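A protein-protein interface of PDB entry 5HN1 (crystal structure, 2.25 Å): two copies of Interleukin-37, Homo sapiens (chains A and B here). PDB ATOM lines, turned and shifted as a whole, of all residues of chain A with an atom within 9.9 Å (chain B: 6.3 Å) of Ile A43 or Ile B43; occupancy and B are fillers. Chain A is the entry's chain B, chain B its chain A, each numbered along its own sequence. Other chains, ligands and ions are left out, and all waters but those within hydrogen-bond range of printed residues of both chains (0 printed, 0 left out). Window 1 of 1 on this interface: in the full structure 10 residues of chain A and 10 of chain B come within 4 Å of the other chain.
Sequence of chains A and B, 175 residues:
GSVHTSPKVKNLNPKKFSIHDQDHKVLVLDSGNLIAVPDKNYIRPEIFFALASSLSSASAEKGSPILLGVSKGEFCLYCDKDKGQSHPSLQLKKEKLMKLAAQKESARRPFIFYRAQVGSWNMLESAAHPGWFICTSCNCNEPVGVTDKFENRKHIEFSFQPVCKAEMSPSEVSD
The side-chain amino group of Lys B40 is in salt-bridge range of the side-chain carboxylate of Asp A30 (3.4 Å).
NH2 of Arg A44 is in hydrogen-bond range of O of Asn B41, 2.8 Å away.
The side-chain carboxylate of Asp A30 lies close to the side-chain hydroxyl of Tyr B42, at 3.5 Å.
The backbone carbonyl oxygen of Tyr B42 is in hydrogen-bond range of the backbone NH of Arg A44, at 2.7 Å.
O of Ile B43 is in hydrogen-bond range of NH2 of Arg A44, 2.8 Å away.
The backbone carbonyl oxygen (O) of Tyr A42 sits at hydrogen-bond distance from the backbone NH (N) of Arg B44, at 2.7 Å.
The guanidinium group (NH1) of Arg B44 sits at hydrogen-bond distance from the backbone carbonyl oxygen (O) of Ile A43, 3.3 Å away.
O of Val B37 is in hydrogen-bond range of N of Val B26 (2.8 Å).
The backbone carbonyl oxygen of Val A28 is in hydrogen-bond range of the backbone NH of Ile A35, at 2.9 Å.
The backbone NH of Asn A141 sits at hydrogen-bond distance from the backbone carbonyl oxygen of Ala A36 (2.9 Å).
Among the printed residues, merely in contact across the chains: Val A28 with Tyr B42 (3.7 Å), Leu A29 with Tyr B42 (3.6 Å), Tyr A42 with Val B28 (3.6 Å), Tyr A42 with Val B37 (3.9 Å), Tyr A42 with Tyr B42 (3.7 Å), Tyr A42 with Ile B43 (3.5 Å), Ile A43 with Tyr B42 (3.5 Å), Ile A43 with Ile B43 (3.6 Å), Arg A44 with Arg B44 (3.6 Å) and Asn A141 with Tyr B42 (3.9 Å).
Ser A18 touches none of the printed residues of chain B.
Of the printed residues of chain B, Asp A30 touches Lys B40 (3.3 Å) and Tyr B42 (3.3 Å).
Ile A43 touches three residues of chain B.
Asp B39 touches none of the printed residues of chain A.
Printed residues of chain A within 4 Å of Asn B41: Arg A44.
Of chain A, only Val A28 (3.7 Å), Leu A29 (3.6 Å), Asp A30 (3.3 Å), Tyr A42 (3.7 Å), Ile A43 (3.5 Å), Arg A44 (2.7 Å) and Asn A141 (3.9 Å) come within 4 Å of Tyr B42.
Ile B43 touches just these residues of chain A: Tyr A42, Ile A43 and Arg A44.
The nearest printed residue of chain B that does not touch Ile A43 is Val B37 (6.8 Å).
The nearest printed residue of chain B that does not touch Tyr A42 is Pro B45 (5.4 Å).
Hydrophobic or aromatic side chains of chain B that line the printed part of chain A: Val B28, Val B37, Tyr B42 and Ile B43.
Hydrophobic or aromatic side chains of chain A that line the printed part of chain B: Val A28, Tyr A42 and Ile A43.
Among the printed residues, 17 pairs touch across the chains.
Tyr A42 touches Val B37, but with the chains exchanged Val A37 does not touch Tyr B42 (4.3 Å).
Tyr A42 touches its own counterpart, Tyr B42.
Ile B43 touches its own counterpart, Ile A43.
Arg A44 touches Asn B41, but with the chains exchanged Asn A41 does not touch Arg B44 (4.003 Å).
Of the 17 pairs that touch across the chains among the printed residues, 11 have their exchanged pair printed and touching as well.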
ATOM      1  N   SER A  18      21.243 -15.842  13.560  1.00  0.00           N
ATOM      2  CA  SER A  18      20.246 -14.852  13.932  1.00  0.00           C
ATOM      3  C   SER A  18      19.241 -15.574  14.818  1.00  0.00           C
ATOM      4  O   SER A  18      19.223 -16.816  14.834  1.00  0.00           O
ATOM      5  CB  SER A  18      19.598 -14.215  12.700  1.00  0.00           C
ATOM      6  OG  SER A  18      18.882 -15.147  11.905  1.00  0.00           O
ATOM      7  N   ILE A  19      18.466 -14.819  15.616  1.00  0.00           N
ATOM      8  CA  ILE A  19      17.494 -15.410  16.546  1.00  0.00           C
ATOM      9  C   ILE A  19      16.101 -14.892  16.192  1.00  0.00           C
ATOM     10  O   ILE A  19      15.852 -13.689  16.208  1.00  0.00           O
ATOM     11  CB  ILE A  19      17.886 -15.170  18.049  1.00  0.00           C
ATOM     12  CG1 ILE A  19      19.224 -15.871  18.381  1.00  0.00           C
ATOM     13  CG2 ILE A  19      16.766 -15.609  19.030  1.00  0.00           C
ATOM     14  CD1 ILE A  19      19.821 -15.619  19.798  1.00  0.00           C
ATOM     15  N   HIS A  20      15.208 -15.834  15.872  1.00  0.00           N
ATOM     16  CA  HIS A  20      13.800 -15.625  15.533  1.00  0.00           C
ATOM     17  C   HIS A  20      12.918 -16.320  16.570  1.00  0.00           C
ATOM     18  O   HIS A  20      13.250 -17.421  16.991  1.00  0.00           O
ATOM     19  CB  HIS A  20      13.497 -16.184  14.132  1.00  0.00           C
ATOM     20  CG  HIS A  20      14.332 -15.591  13.040  1.00  0.00           C
ATOM     21  ND1 HIS A  20      13.787 -14.721  12.105  1.00  0.00           N
ATOM     22  CD2 HIS A  20      15.653 -15.744  12.777  1.00  0.00           C
ATOM     23  CE1 HIS A  20      14.784 -14.398  11.295  1.00  0.00           C
ATOM     24  NE2 HIS A  20      15.930 -14.962  11.677  1.00  0.00           N
ATOM     25  N   HIS A  24       7.429 -14.898  14.533  1.00  0.00           N
ATOM     26  CA  HIS A  24       8.250 -14.490  13.380  1.00  0.00           C
ATOM     27  C   HIS A  24       8.957 -13.132  13.646  1.00  0.00           C
ATOM     28  O   HIS A  24       9.254 -12.387  12.696  1.00  0.00           O
ATOM     29  CB  HIS A  24       7.440 -14.449  12.050  1.00  0.00           C
ATOM     30  CG  HIS A  24       6.746 -15.729  11.677  1.00  0.00           C
ATOM     31  ND1 HIS A  24       7.425 -16.945  11.635  1.00  0.00           N
ATOM     32  CD2 HIS A  24       5.459 -15.936  11.305  1.00  0.00           C
ATOM     33  CE1 HIS A  24       6.523 -17.844  11.270  1.00  0.00           C
ATOM     34  NE2 HIS A  24       5.328 -17.285  11.056  1.00  0.00           N
ATOM     35  N   LYS A  25       9.203 -12.799  14.935  1.00  0.00           N
ATOM     36  CA  LYS A  25       9.940 -11.584  15.290  1.00  0.00           C
ATOM     37  C   LYS A  25      11.426 -11.948  15.323  1.00  0.00           C
ATOM     38  O   LYS A  25      11.769 -13.103  15.589  1.00  0.00           O
ATOM     39  CB  LYS A  25       9.466 -10.955  16.609  1.00  0.00           C
ATOM     40  CG  LYS A  25       8.030 -10.413  16.559  1.00  0.00           C
ATOM     41  CD  LYS A  25       7.686  -9.399  17.674  1.00  0.00           C
ATOM     42  CE  LYS A  25       8.015  -9.828  19.103  1.00  0.00           C
ATOM     43  NZ  LYS A  25       7.390 -11.126  19.503  1.00  0.00           N
ATOM     44  N   VAL A  26      12.299 -10.997  14.993  1.00  0.00           N
ATOM     45  CA  VAL A  26      13.740 -11.249  14.939  1.00  0.00           C
ATOM     46  C   VAL A  26      14.448 -10.273  15.918  1.00  0.00           C
ATOM     47  O   VAL A  26      13.923  -9.202  16.225  1.00  0.00           O
ATOM     48  CB  VAL A  26      14.289 -11.202  13.470  1.00  0.00           C
ATOM     49  CG1 VAL A  26      14.254  -9.805  12.876  1.00  0.00           C
ATOM     50  CG2 VAL A  26      15.691 -11.789  13.374  1.00  0.00           C
ATOM     51  N   LEU A  27      15.604 -10.678  16.434  1.00  0.00           N
ATOM     52  CA  LEU A  27      16.359  -9.883  17.392  1.00  0.00           C
ATOM     53  C   LEU A  27      17.325  -8.992  16.683  1.00  0.00           C
ATOM     54  O   LEU A  27      18.061  -9.427  15.794  1.00  0.00           O
ATOM     55  CB  LEU A  27      17.091 -10.775  18.409  1.00  0.00           C
ATOM     56  CG  LEU A  27      16.324 -11.127  19.681  1.00  0.00           C
ATOM     57  CD1 LEU A  27      14.966 -11.760  19.374  1.00  0.00           C
ATOM     58  CD2 LEU A  27      17.132 -12.077  20.556  1.00  0.00           C
ATOM     59  N   VAL A  28      17.251  -7.711  17.032  1.00  0.00           N
ATOM     60  CA  VAL A  28      18.076  -6.637  16.502  1.00  0.00           C
ATOM     61  C   VAL A  28      18.558  -5.815  17.686  1.00  0.00           C
ATOM     62  O   VAL A  28      17.961  -5.869  18.771  1.00  0.00           O
ATOM     63  CB  VAL A  28      17.357  -5.761  15.417  1.00  0.00           C
ATOM     64  CG1 VAL A  28      16.962  -6.584  14.193  1.00  0.00           C
ATOM     65  CG2 VAL A  28      16.146  -5.013  15.982  1.00  0.00           C
ATOM     66  N   LEU A  29      19.635  -5.062  17.469  1.00  0.00           N
ATOM     67  CA  LEU A  29      20.232  -4.172  18.451  1.00  0.00           C
ATOM     68  C   LEU A  29      19.774  -2.750  18.143  1.00  0.00           C
ATOM     69  O   LEU A  29      19.997  -2.263  17.037  1.00  0.00           O
ATOM     70  CB  LEU A  29      21.766  -4.309  18.383  1.00  0.00           C
ATOM     71  CG  LEU A  29      22.615  -3.866  19.589  1.00  0.00           C
ATOM     72  CD1 LEU A  29      22.264  -4.647  20.840  1.00  0.00           C
ATOM     73  CD2 LEU A  29      24.077  -4.127  19.310  1.00  0.00           C
ATOM     74  N   ASP A  30      19.070  -2.120  19.105  1.00  0.00           N
ATOM     75  CA  ASP A  30      18.520  -0.763  19.011  1.00  0.00           C
ATOM     76  C   ASP A  30      19.051   0.109  20.152  1.00  0.00           C
ATOM     77  O   ASP A  30      18.661  -0.083  21.310  1.00  0.00           O
ATOM     78  CB  ASP A  30      16.984  -0.803  19.042  1.00  0.00           C
ATOM     79  CG  ASP A  30      16.327   0.544  18.796  1.00  0.00           C
ATOM     80  OD1 ASP A  30      15.929   0.804  17.649  1.00  0.00           O
ATOM     81  OD2 ASP A  30      16.175   1.313  19.761  1.00  0.00           O
ATOM     82  N   ILE A  35      16.161  -5.860  21.055  1.00  0.00           N
ATOM     83  CA  ILE A  35      14.698  -5.793  20.918  1.00  0.00           C
ATOM     84  C   ILE A  35      14.246  -6.813  19.870  1.00  0.00           C
ATOM     85  O   ILE A  35      15.056  -7.202  19.026  1.00  0.00           O
ATOM     86  CB  ILE A  35      14.154  -4.352  20.598  1.00  0.00           C
ATOM     87  CG1 ILE A  35      14.667  -3.780  19.242  1.00  0.00           C
ATOM     88  CG2 ILE A  35      14.393  -3.378  21.758  1.00  0.00           C
ATOM     89  CD1 ILE A  35      13.836  -2.560  18.663  1.00  0.00           C
ATOM     90  N   ALA A  36      12.950  -7.210  19.896  1.00  0.00           N
ATOM     91  CA  ALA A  36      12.359  -8.128  18.914  1.00  0.00           C
ATOM     92  C   ALA A  36      11.412  -7.353  17.980  1.00  0.00           C
ATOM     93  O   ALA A  36      10.468  -6.695  18.436  1.00  0.00           O
ATOM     94  CB  ALA A  36      11.637  -9.285  19.599  1.00  0.00           C
ATOM     95  N   VAL A  37      11.724  -7.369  16.678  1.00  0.00           N
ATOM     96  CA  VAL A  37      10.964  -6.606  15.678  1.00  0.00           C
ATOM     97  C   VAL A  37      10.376  -7.555  14.628  1.00  0.00           C
ATOM     98  O   VAL A  37      11.008  -8.566  14.327  1.00  0.00           O
ATOM     99  CB  VAL A  37      11.824  -5.464  15.026  1.00  0.00           C
ATOM    100  CG1 VAL A  37      12.302  -4.469  16.070  1.00  0.00           C
ATOM    101  CG2 VAL A  37      13.010  -6.000  14.227  1.00  0.00           C
ATOM    102  N   PRO A  38       9.181  -7.273  14.061  1.00  0.00           N
ATOM    103  CA  PRO A  38       8.665  -8.155  12.985  1.00  0.00           C
ATOM    104  C   PRO A  38       9.708  -8.294  11.878  1.00  0.00           C
ATOM    105  O   PRO A  38      10.263  -7.278  11.453  1.00  0.00           O
ATOM    106  CB  PRO A  38       7.412  -7.418  12.472  1.00  0.00           C
ATOM    107  CG  PRO A  38       7.076  -6.423  13.511  1.00  0.00           C
ATOM    108  CD  PRO A  38       8.323  -6.080  14.248  1.00  0.00           C
ATOM    109  N   ASP A  39      10.059  -9.531  11.491  1.00  0.00           N
ATOM    110  CA  ASP A  39      11.093  -9.726  10.473  1.00  0.00           C
ATOM    111  C   ASP A  39      10.561  -9.319   9.114  1.00  0.00           C
ATOM    112  O   ASP A  39       9.448  -9.688   8.741  1.00  0.00           O
ATOM    113  CB  ASP A  39      11.631 -11.168  10.460  1.00  0.00           C
ATOM    114  CG  ASP A  39      12.925 -11.365   9.669  1.00  0.00           C
ATOM    115  OD1 ASP A  39      13.589 -10.344   9.330  1.00  0.00           O
ATOM    116  OD2 ASP A  39      13.269 -12.530   9.375  1.00  0.00           O
ATOM    117  N   LYS A  40      11.324  -8.462   8.424  1.00  0.00           N
ATOM    118  CA  LYS A  40      11.011  -7.916   7.110  1.00  0.00           C
ATOM    119  C   LYS A  40      12.243  -7.995   6.232  1.00  0.00           C
ATOM    120  O   LYS A  40      13.347  -8.134   6.748  1.00  0.00           O
ATOM    121  CB  LYS A  40      10.540  -6.443   7.238  1.00  0.00           C
ATOM    122  CG  LYS A  40       9.283  -6.218   8.081  1.00  0.00           C
ATOM    123  CD  LYS A  40       8.003  -6.426   7.283  1.00  0.00           C
ATOM    124  CE  LYS A  40       6.797  -6.279   8.166  1.00  0.00           C
ATOM    125  NZ  LYS A  40       5.538  -6.438   7.395  1.00  0.00           N
ATOM    126  N   ASN A  41      12.064  -7.874   4.915  1.00  0.00           N
ATOM    127  CA  ASN A  41      13.134  -7.859   3.907  1.00  0.00           C
ATOM    128  C   ASN A  41      14.186  -6.748   4.197  1.00  0.00           C
ATOM    129  O   ASN A  41      15.379  -6.951   3.982  1.00  0.00           O
ATOM    130  CB  ASN A  41      12.519  -7.647   2.494  1.00  0.00           C
ATOM    131  CG  ASN A  41      11.509  -6.505   2.392  1.00  0.00           C
ATOM    132  OD1 ASN A  41      11.833  -5.381   1.997  1.00  0.00           O
ATOM    133  ND2 ASN A  41      10.246  -6.768   2.725  1.00  0.00           N
ATOM    134  N   TYR A  42      13.730  -5.589   4.696  1.00  0.00           N
ATOM    135  CA  TYR A  42      14.587  -4.434   4.982  1.00  0.00           C
ATOM    136  C   TYR A  42      15.268  -4.490   6.361  1.00  0.00           C
ATOM    137  O   TYR A  42      16.008  -3.560   6.717  1.00  0.00           O
ATOM    138  CB  TYR A  42      13.799  -3.131   4.850  1.00  0.00           C
ATOM    139  CG  TYR A  42      12.507  -3.042   5.630  1.00  0.00           C
ATOM    140  CD1 TYR A  42      12.496  -2.601   6.953  1.00  0.00           C
ATOM    141  CD2 TYR A  42      11.281  -3.258   5.007  1.00  0.00           C
ATOM    142  CE1 TYR A  42      11.299  -2.413   7.645  1.00  0.00           C
ATOM    143  CE2 TYR A  42      10.078  -3.067   5.686  1.00  0.00           C
ATOM    144  CZ  TYR A  42      10.091  -2.662   7.010  1.00  0.00           C
ATOM    145  OH  TYR A  42       8.901  -2.471   7.670  1.00  0.00           O
ATOM    146  N   ILE A  43      15.015  -5.561   7.126  1.00  0.00           N
ATOM    147  CA  ILE A  43      15.595  -5.740   8.443  1.00  0.00           C
ATOM    148  C   ILE A  43      16.888  -6.541   8.343  1.00  0.00           C
ATOM    149  O   ILE A  43      16.934  -7.588   7.699  1.00  0.00           O
ATOM    150  CB  ILE A  43      14.593  -6.423   9.427  1.00  0.00           C
ATOM    151  CG1 ILE A  43      13.297  -5.583   9.647  1.00  0.00           C
ATOM    152  CG2 ILE A  43      15.266  -6.828  10.733  1.00  0.00           C
ATOM    153  CD1 ILE A  43      13.417  -4.294  10.479  1.00  0.00           C
ATOM    154  N   ARG A  44      17.917  -6.050   9.033  1.00  0.00           N
ATOM    155  CA  ARG A  44      19.220  -6.665   9.169  1.00  0.00           C
ATOM    156  C   ARG A  44      19.258  -7.306  10.576  1.00  0.00           C
ATOM    157  O   ARG A  44      19.392  -6.593  11.585  1.00  0.00           O
ATOM    158  CB  ARG A  44      20.301  -5.596   8.960  1.00  0.00           C
ATOM    159  CG  ARG A  44      21.715  -6.158   8.773  1.00  0.00           C
ATOM    160  CD  ARG A  44      22.549  -5.380   7.752  1.00  0.00           C
ATOM    161  NE  ARG A  44      22.103  -3.999   7.531  1.00  0.00           N
ATOM    162  CZ  ARG A  44      22.470  -2.959   8.274  1.00  0.00           C
ATOM    163  NH1 ARG A  44      23.265  -3.133   9.325  1.00  0.00           N
ATOM    164  NH2 ARG A  44      22.020  -1.741   7.992  1.00  0.00           N
ATOM    165  N   PRO A  45      19.018  -8.634  10.674  1.00  0.00           N
ATOM    166  CA  PRO A  45      18.995  -9.278  12.002  1.00  0.00           C
ATOM    167  C   PRO A  45      20.327  -9.200  12.710  1.00  0.00           C
ATOM    168  O   PRO A  45      21.362  -9.229  12.047  1.00  0.00           O
ATOM    169  CB  PRO A  45      18.674 -10.744  11.685  1.00  0.00           C
ATOM    170  CG  PRO A  45      18.112 -10.745  10.314  1.00  0.00           C
ATOM    171  CD  PRO A  45      18.810  -9.626   9.599  1.00  0.00           C
ATOM    172  N   GLU A  46      20.312  -9.095  14.046  1.00  0.00           N
ATOM    173  CA  GLU A  46      21.558  -9.115  14.802  1.00  0.00           C
ATOM    174  C   GLU A  46      22.186 -10.519  14.670  1.00  0.00           C
ATOM    175  O   GLU A  46      21.468 -11.514  14.803  1.00  0.00           O
ATOM    176  CB  GLU A  46      21.316  -8.765  16.283  1.00  0.00           C
ATOM    177  CG  GLU A  46      22.565  -8.859  17.160  1.00  0.00           C
ATOM    178  CD  GLU A  46      23.731  -7.974  16.741  1.00  0.00           C
ATOM    179  OE1 GLU A  46      24.888  -8.448  16.821  1.00  0.00           O
ATOM    180  OE2 GLU A  46      23.490  -6.822  16.309  1.00  0.00           O
ATOM    181  N   ILE A  47      23.497 -10.584  14.374  1.00  0.00           N
ATOM    182  CA  ILE A  47      24.209 -11.854  14.264  1.00  0.00           C
ATOM    183  C   ILE A  47      24.855 -12.187  15.625  1.00  0.00           C
ATOM    184  O   ILE A  47      25.715 -11.459  16.133  1.00  0.00           O
ATOM    185  CB  ILE A  47      25.207 -11.923  13.068  1.00  0.00           C
ATOM    186  CG1 ILE A  47      24.494 -11.623  11.714  1.00  0.00           C
ATOM    187  CG2 ILE A  47      25.975 -13.285  13.033  1.00  0.00           C
ATOM    188  CD1 ILE A  47      23.334 -12.621  11.329  1.00  0.00           C
ATOM    189  N   ASN A 141       8.789  -4.406  18.975  1.00  0.00           N
ATOM    190  CA  ASN A 141       9.736  -3.356  19.360  1.00  0.00           C
ATOM    191  C   ASN A 141       9.862  -3.164  20.887  1.00  0.00           C
ATOM    192  O   ASN A 141      10.029  -2.038  21.367  1.00  0.00           O
ATOM    193  CB  ASN A 141       9.362  -2.045  18.664  1.00  0.00           C
ATOM    194  CG  ASN A 141       9.639  -2.045  17.175  1.00  0.00           C
ATOM    195  OD1 ASN A 141      10.502  -1.306  16.681  1.00  0.00           O
ATOM    196  ND2 ASN A 141       8.909  -2.866  16.419  1.00  0.00           N
ATOM    197  N   VAL B  26      13.782   6.696   7.090  1.00  0.00           N
ATOM    198  CA  VAL B  26      14.445   6.277   5.856  1.00  0.00           C
ATOM    199  C   VAL B  26      13.416   5.489   5.007  1.00  0.00           C
ATOM    200  O   VAL B  26      12.559   4.772   5.554  1.00  0.00           O
ATOM    201  CB  VAL B  26      15.757   5.480   6.145  1.00  0.00           C
ATOM    202  CG1 VAL B  26      15.501   4.184   6.923  1.00  0.00           C
ATOM    203  CG2 VAL B  26      16.566   5.219   4.879  1.00  0.00           C
ATOM    204  N   LEU B  27      13.532   5.597   3.685  1.00  0.00           N
ATOM    205  CA  LEU B  27      12.626   4.928   2.747  1.00  0.00           C
ATOM    206  C   LEU B  27      13.078   3.513   2.422  1.00  0.00           C
ATOM    207  O   LEU B  27      14.260   3.272   2.150  1.00  0.00           O
ATOM    208  CB  LEU B  27      12.484   5.745   1.461  1.00  0.00           C
ATOM    209  CG  LEU B  27      11.486   6.926   1.444  1.00  0.00           C
ATOM    210  CD1 LEU B  27      11.623   7.808   2.635  1.00  0.00           C
ATOM    211  CD2 LEU B  27      11.637   7.772   0.116  1.00  0.00           C
ATOM    212  N   VAL B  28      12.125   2.572   2.487  1.00  0.00           N
ATOM    213  CA  VAL B  28      12.333   1.154   2.207  1.00  0.00           C
ATOM    214  C   VAL B  28      11.148   0.648   1.377  1.00  0.00           C
ATOM    215  O   VAL B  28      10.073   1.265   1.353  1.00  0.00           O
ATOM    216  CB  VAL B  28      12.561   0.268   3.492  1.00  0.00           C
ATOM    217  CG1 VAL B  28      13.808   0.697   4.277  1.00  0.00           C
ATOM    218  CG2 VAL B  28      11.337   0.254   4.409  1.00  0.00           C
ATOM    219  N   VAL B  37      10.373   4.240   7.401  1.00  0.00           N
ATOM    220  CA  VAL B  37      10.510   3.549   8.678  1.00  0.00           C
ATOM    221  C   VAL B  37      11.525   4.325   9.501  1.00  0.00           C
ATOM    222  O   VAL B  37      12.303   5.070   8.898  1.00  0.00           O
ATOM    223  CB  VAL B  37      10.926   2.053   8.477  1.00  0.00           C
ATOM    224  CG1 VAL B  37       9.888   1.295   7.647  1.00  0.00           C
ATOM    225  CG2 VAL B  37      12.322   1.923   7.850  1.00  0.00           C
ATOM    226  N   PRO B  38      11.578   4.175  10.854  1.00  0.00           N
ATOM    227  CA  PRO B  38      12.604   4.920  11.609  1.00  0.00           C
ATOM    228  C   PRO B  38      14.013   4.517  11.138  1.00  0.00           C
ATOM    229  O   PRO B  38      14.286   3.359  10.810  1.00  0.00           O
ATOM    230  CB  PRO B  38      12.323   4.561  13.081  1.00  0.00           C
ATOM    231  CG  PRO B  38      11.497   3.319  13.034  1.00  0.00           C
ATOM    232  CD  PRO B  38      10.748   3.321  11.740  1.00  0.00           C
ATOM    233  N   ASP B  39      14.864   5.522  10.994  1.00  0.00           N
ATOM    234  CA  ASP B  39      16.225   5.400  10.496  1.00  0.00           C
ATOM    235  C   ASP B  39      17.147   4.814  11.563  1.00  0.00           C
ATOM    236  O   ASP B  39      17.782   5.556  12.306  1.00  0.00           O
ATOM    237  CB  ASP B  39      16.682   6.799  10.070  1.00  0.00           C
ATOM    238  CG  ASP B  39      17.914   6.900   9.195  1.00  0.00           C
ATOM    239  OD1 ASP B  39      18.692   5.897   9.122  1.00  0.00           O
ATOM    240  OD2 ASP B  39      18.142   8.001   8.631  1.00  0.00           O
ATOM    241  N   LYS B  40      17.218   3.473  11.633  1.00  0.00           N
ATOM    242  CA  LYS B  40      18.031   2.721  12.594  1.00  0.00           C
ATOM    243  C   LYS B  40      19.086   1.860  11.904  1.00  0.00           C
ATOM    244  O   LYS B  40      18.949   1.536  10.726  1.00  0.00           O
ATOM    245  CB  LYS B  40      17.126   1.836  13.475  1.00  0.00           C
ATOM    246  CG  LYS B  40      16.124   2.612  14.345  1.00  0.00           C
ATOM    247  CD  LYS B  40      16.781   3.192  15.599  1.00  0.00           C
ATOM    248  CE  LYS B  40      15.807   3.926  16.491  1.00  0.00           C
ATOM    249  NZ  LYS B  40      16.367   4.145  17.854  1.00  0.00           N
ATOM    250  N   ASN B  41      20.128   1.471  12.658  1.00  0.00           N
ATOM    251  CA  ASN B  41      21.255   0.640  12.217  1.00  0.00           C
ATOM    252  C   ASN B  41      20.825  -0.714  11.632  1.00  0.00           C
ATOM    253  O   ASN B  41      21.497  -1.225  10.739  1.00  0.00           O
ATOM    254  CB  ASN B  41      22.217   0.371  13.402  1.00  0.00           C
ATOM    255  CG  ASN B  41      23.185   1.484  13.757  1.00  0.00           C
ATOM    256  OD1 ASN B  41      23.590   2.308  12.922  1.00  0.00           O
ATOM    257  ND2 ASN B  41      23.633   1.490  15.005  1.00  0.00           N
ATOM    258  N   TYR B  42      19.728  -1.306  12.143  1.00  0.00           N
ATOM    259  CA  TYR B  42      19.254  -2.615  11.681  1.00  0.00           C
ATOM    260  C   TYR B  42      18.416  -2.498  10.401  1.00  0.00           C
ATOM    261  O   TYR B  42      17.885  -3.502   9.926  1.00  0.00           O
ATOM    262  CB  TYR B  42      18.473  -3.360  12.790  1.00  0.00           C
ATOM    263  CG  TYR B  42      17.301  -2.602  13.383  1.00  0.00           C
ATOM    264  CD1 TYR B  42      16.039  -2.664  12.800  1.00  0.00           C
ATOM    265  CD2 TYR B  42      17.437  -1.889  14.569  1.00  0.00           C
ATOM    266  CE1 TYR B  42      14.955  -1.977  13.349  1.00  0.00           C
ATOM    267  CE2 TYR B  42      16.352  -1.235  15.151  1.00  0.00           C
ATOM    268  CZ  TYR B  42      15.115  -1.270  14.528  1.00  0.00           C
ATOM    269  OH  TYR B  42      14.044  -0.625  15.095  1.00  0.00           O
ATOM    270  N   ILE B  43      18.308  -1.291   9.834  1.00  0.00           N
ATOM    271  CA  ILE B  43      17.534  -1.106   8.628  1.00  0.00           C
ATOM    272  C   ILE B  43      18.454  -1.098   7.398  1.00  0.00           C
ATOM    273  O   ILE B  43      19.529  -0.493   7.416  1.00  0.00           O
ATOM    274  CB  ILE B  43      16.646   0.178   8.714  1.00  0.00           C
ATOM    275  CG1 ILE B  43      15.631   0.116   9.912  1.00  0.00           C
ATOM    276  CG2 ILE B  43      15.977   0.527   7.376  1.00  0.00           C
ATOM    277  CD1 ILE B  43      14.492  -0.909   9.812  1.00  0.00           C
ATOM    278  N   ARG B  44      18.024  -1.829   6.355  1.00  0.00           N
ATOM    279  CA  ARG B  44      18.647  -1.905   5.035  1.00  0.00           C
ATOM    280  C   ARG B  44      17.901  -0.887   4.151  1.00  0.00           C
ATOM    281  O   ARG B  44      16.766  -1.151   3.737  1.00  0.00           O
ATOM    282  CB  ARG B  44      18.591  -3.331   4.453  1.00  0.00           C
ATOM    283  CG  ARG B  44      19.343  -4.387   5.266  1.00  0.00           C
ATOM    284  CD  ARG B  44      19.315  -5.774   4.622  1.00  0.00           C
ATOM    285  NE  ARG B  44      20.240  -6.686   5.306  1.00  0.00           N
ATOM    286  CZ  ARG B  44      20.004  -7.974   5.544  1.00  0.00           C
ATOM    287  NH1 ARG B  44      18.867  -8.534   5.146  1.00  0.00           N
ATOM    288  NH2 ARG B  44      20.900  -8.711   6.189  1.00  0.00           N
ATOM    289  N   PRO B  45      18.446   0.334   3.957  1.00  0.00           N
ATOM    290  CA  PRO B  45      17.717   1.342   3.164  1.00  0.00           C
ATOM    291  C   PRO B  45      17.535   0.948   1.710  1.00  0.00           C
ATOM    292  O   PRO B  45      18.341   0.186   1.172  1.00  0.00           O
ATOM    293  CB  PRO B  45      18.628   2.568   3.234  1.00  0.00           C
ATOM    294  CG  PRO B  45      19.508   2.330   4.432  1.00  0.00           C
ATOM    295  CD  PRO B  45      19.746   0.858   4.419  1.00  0.00           C
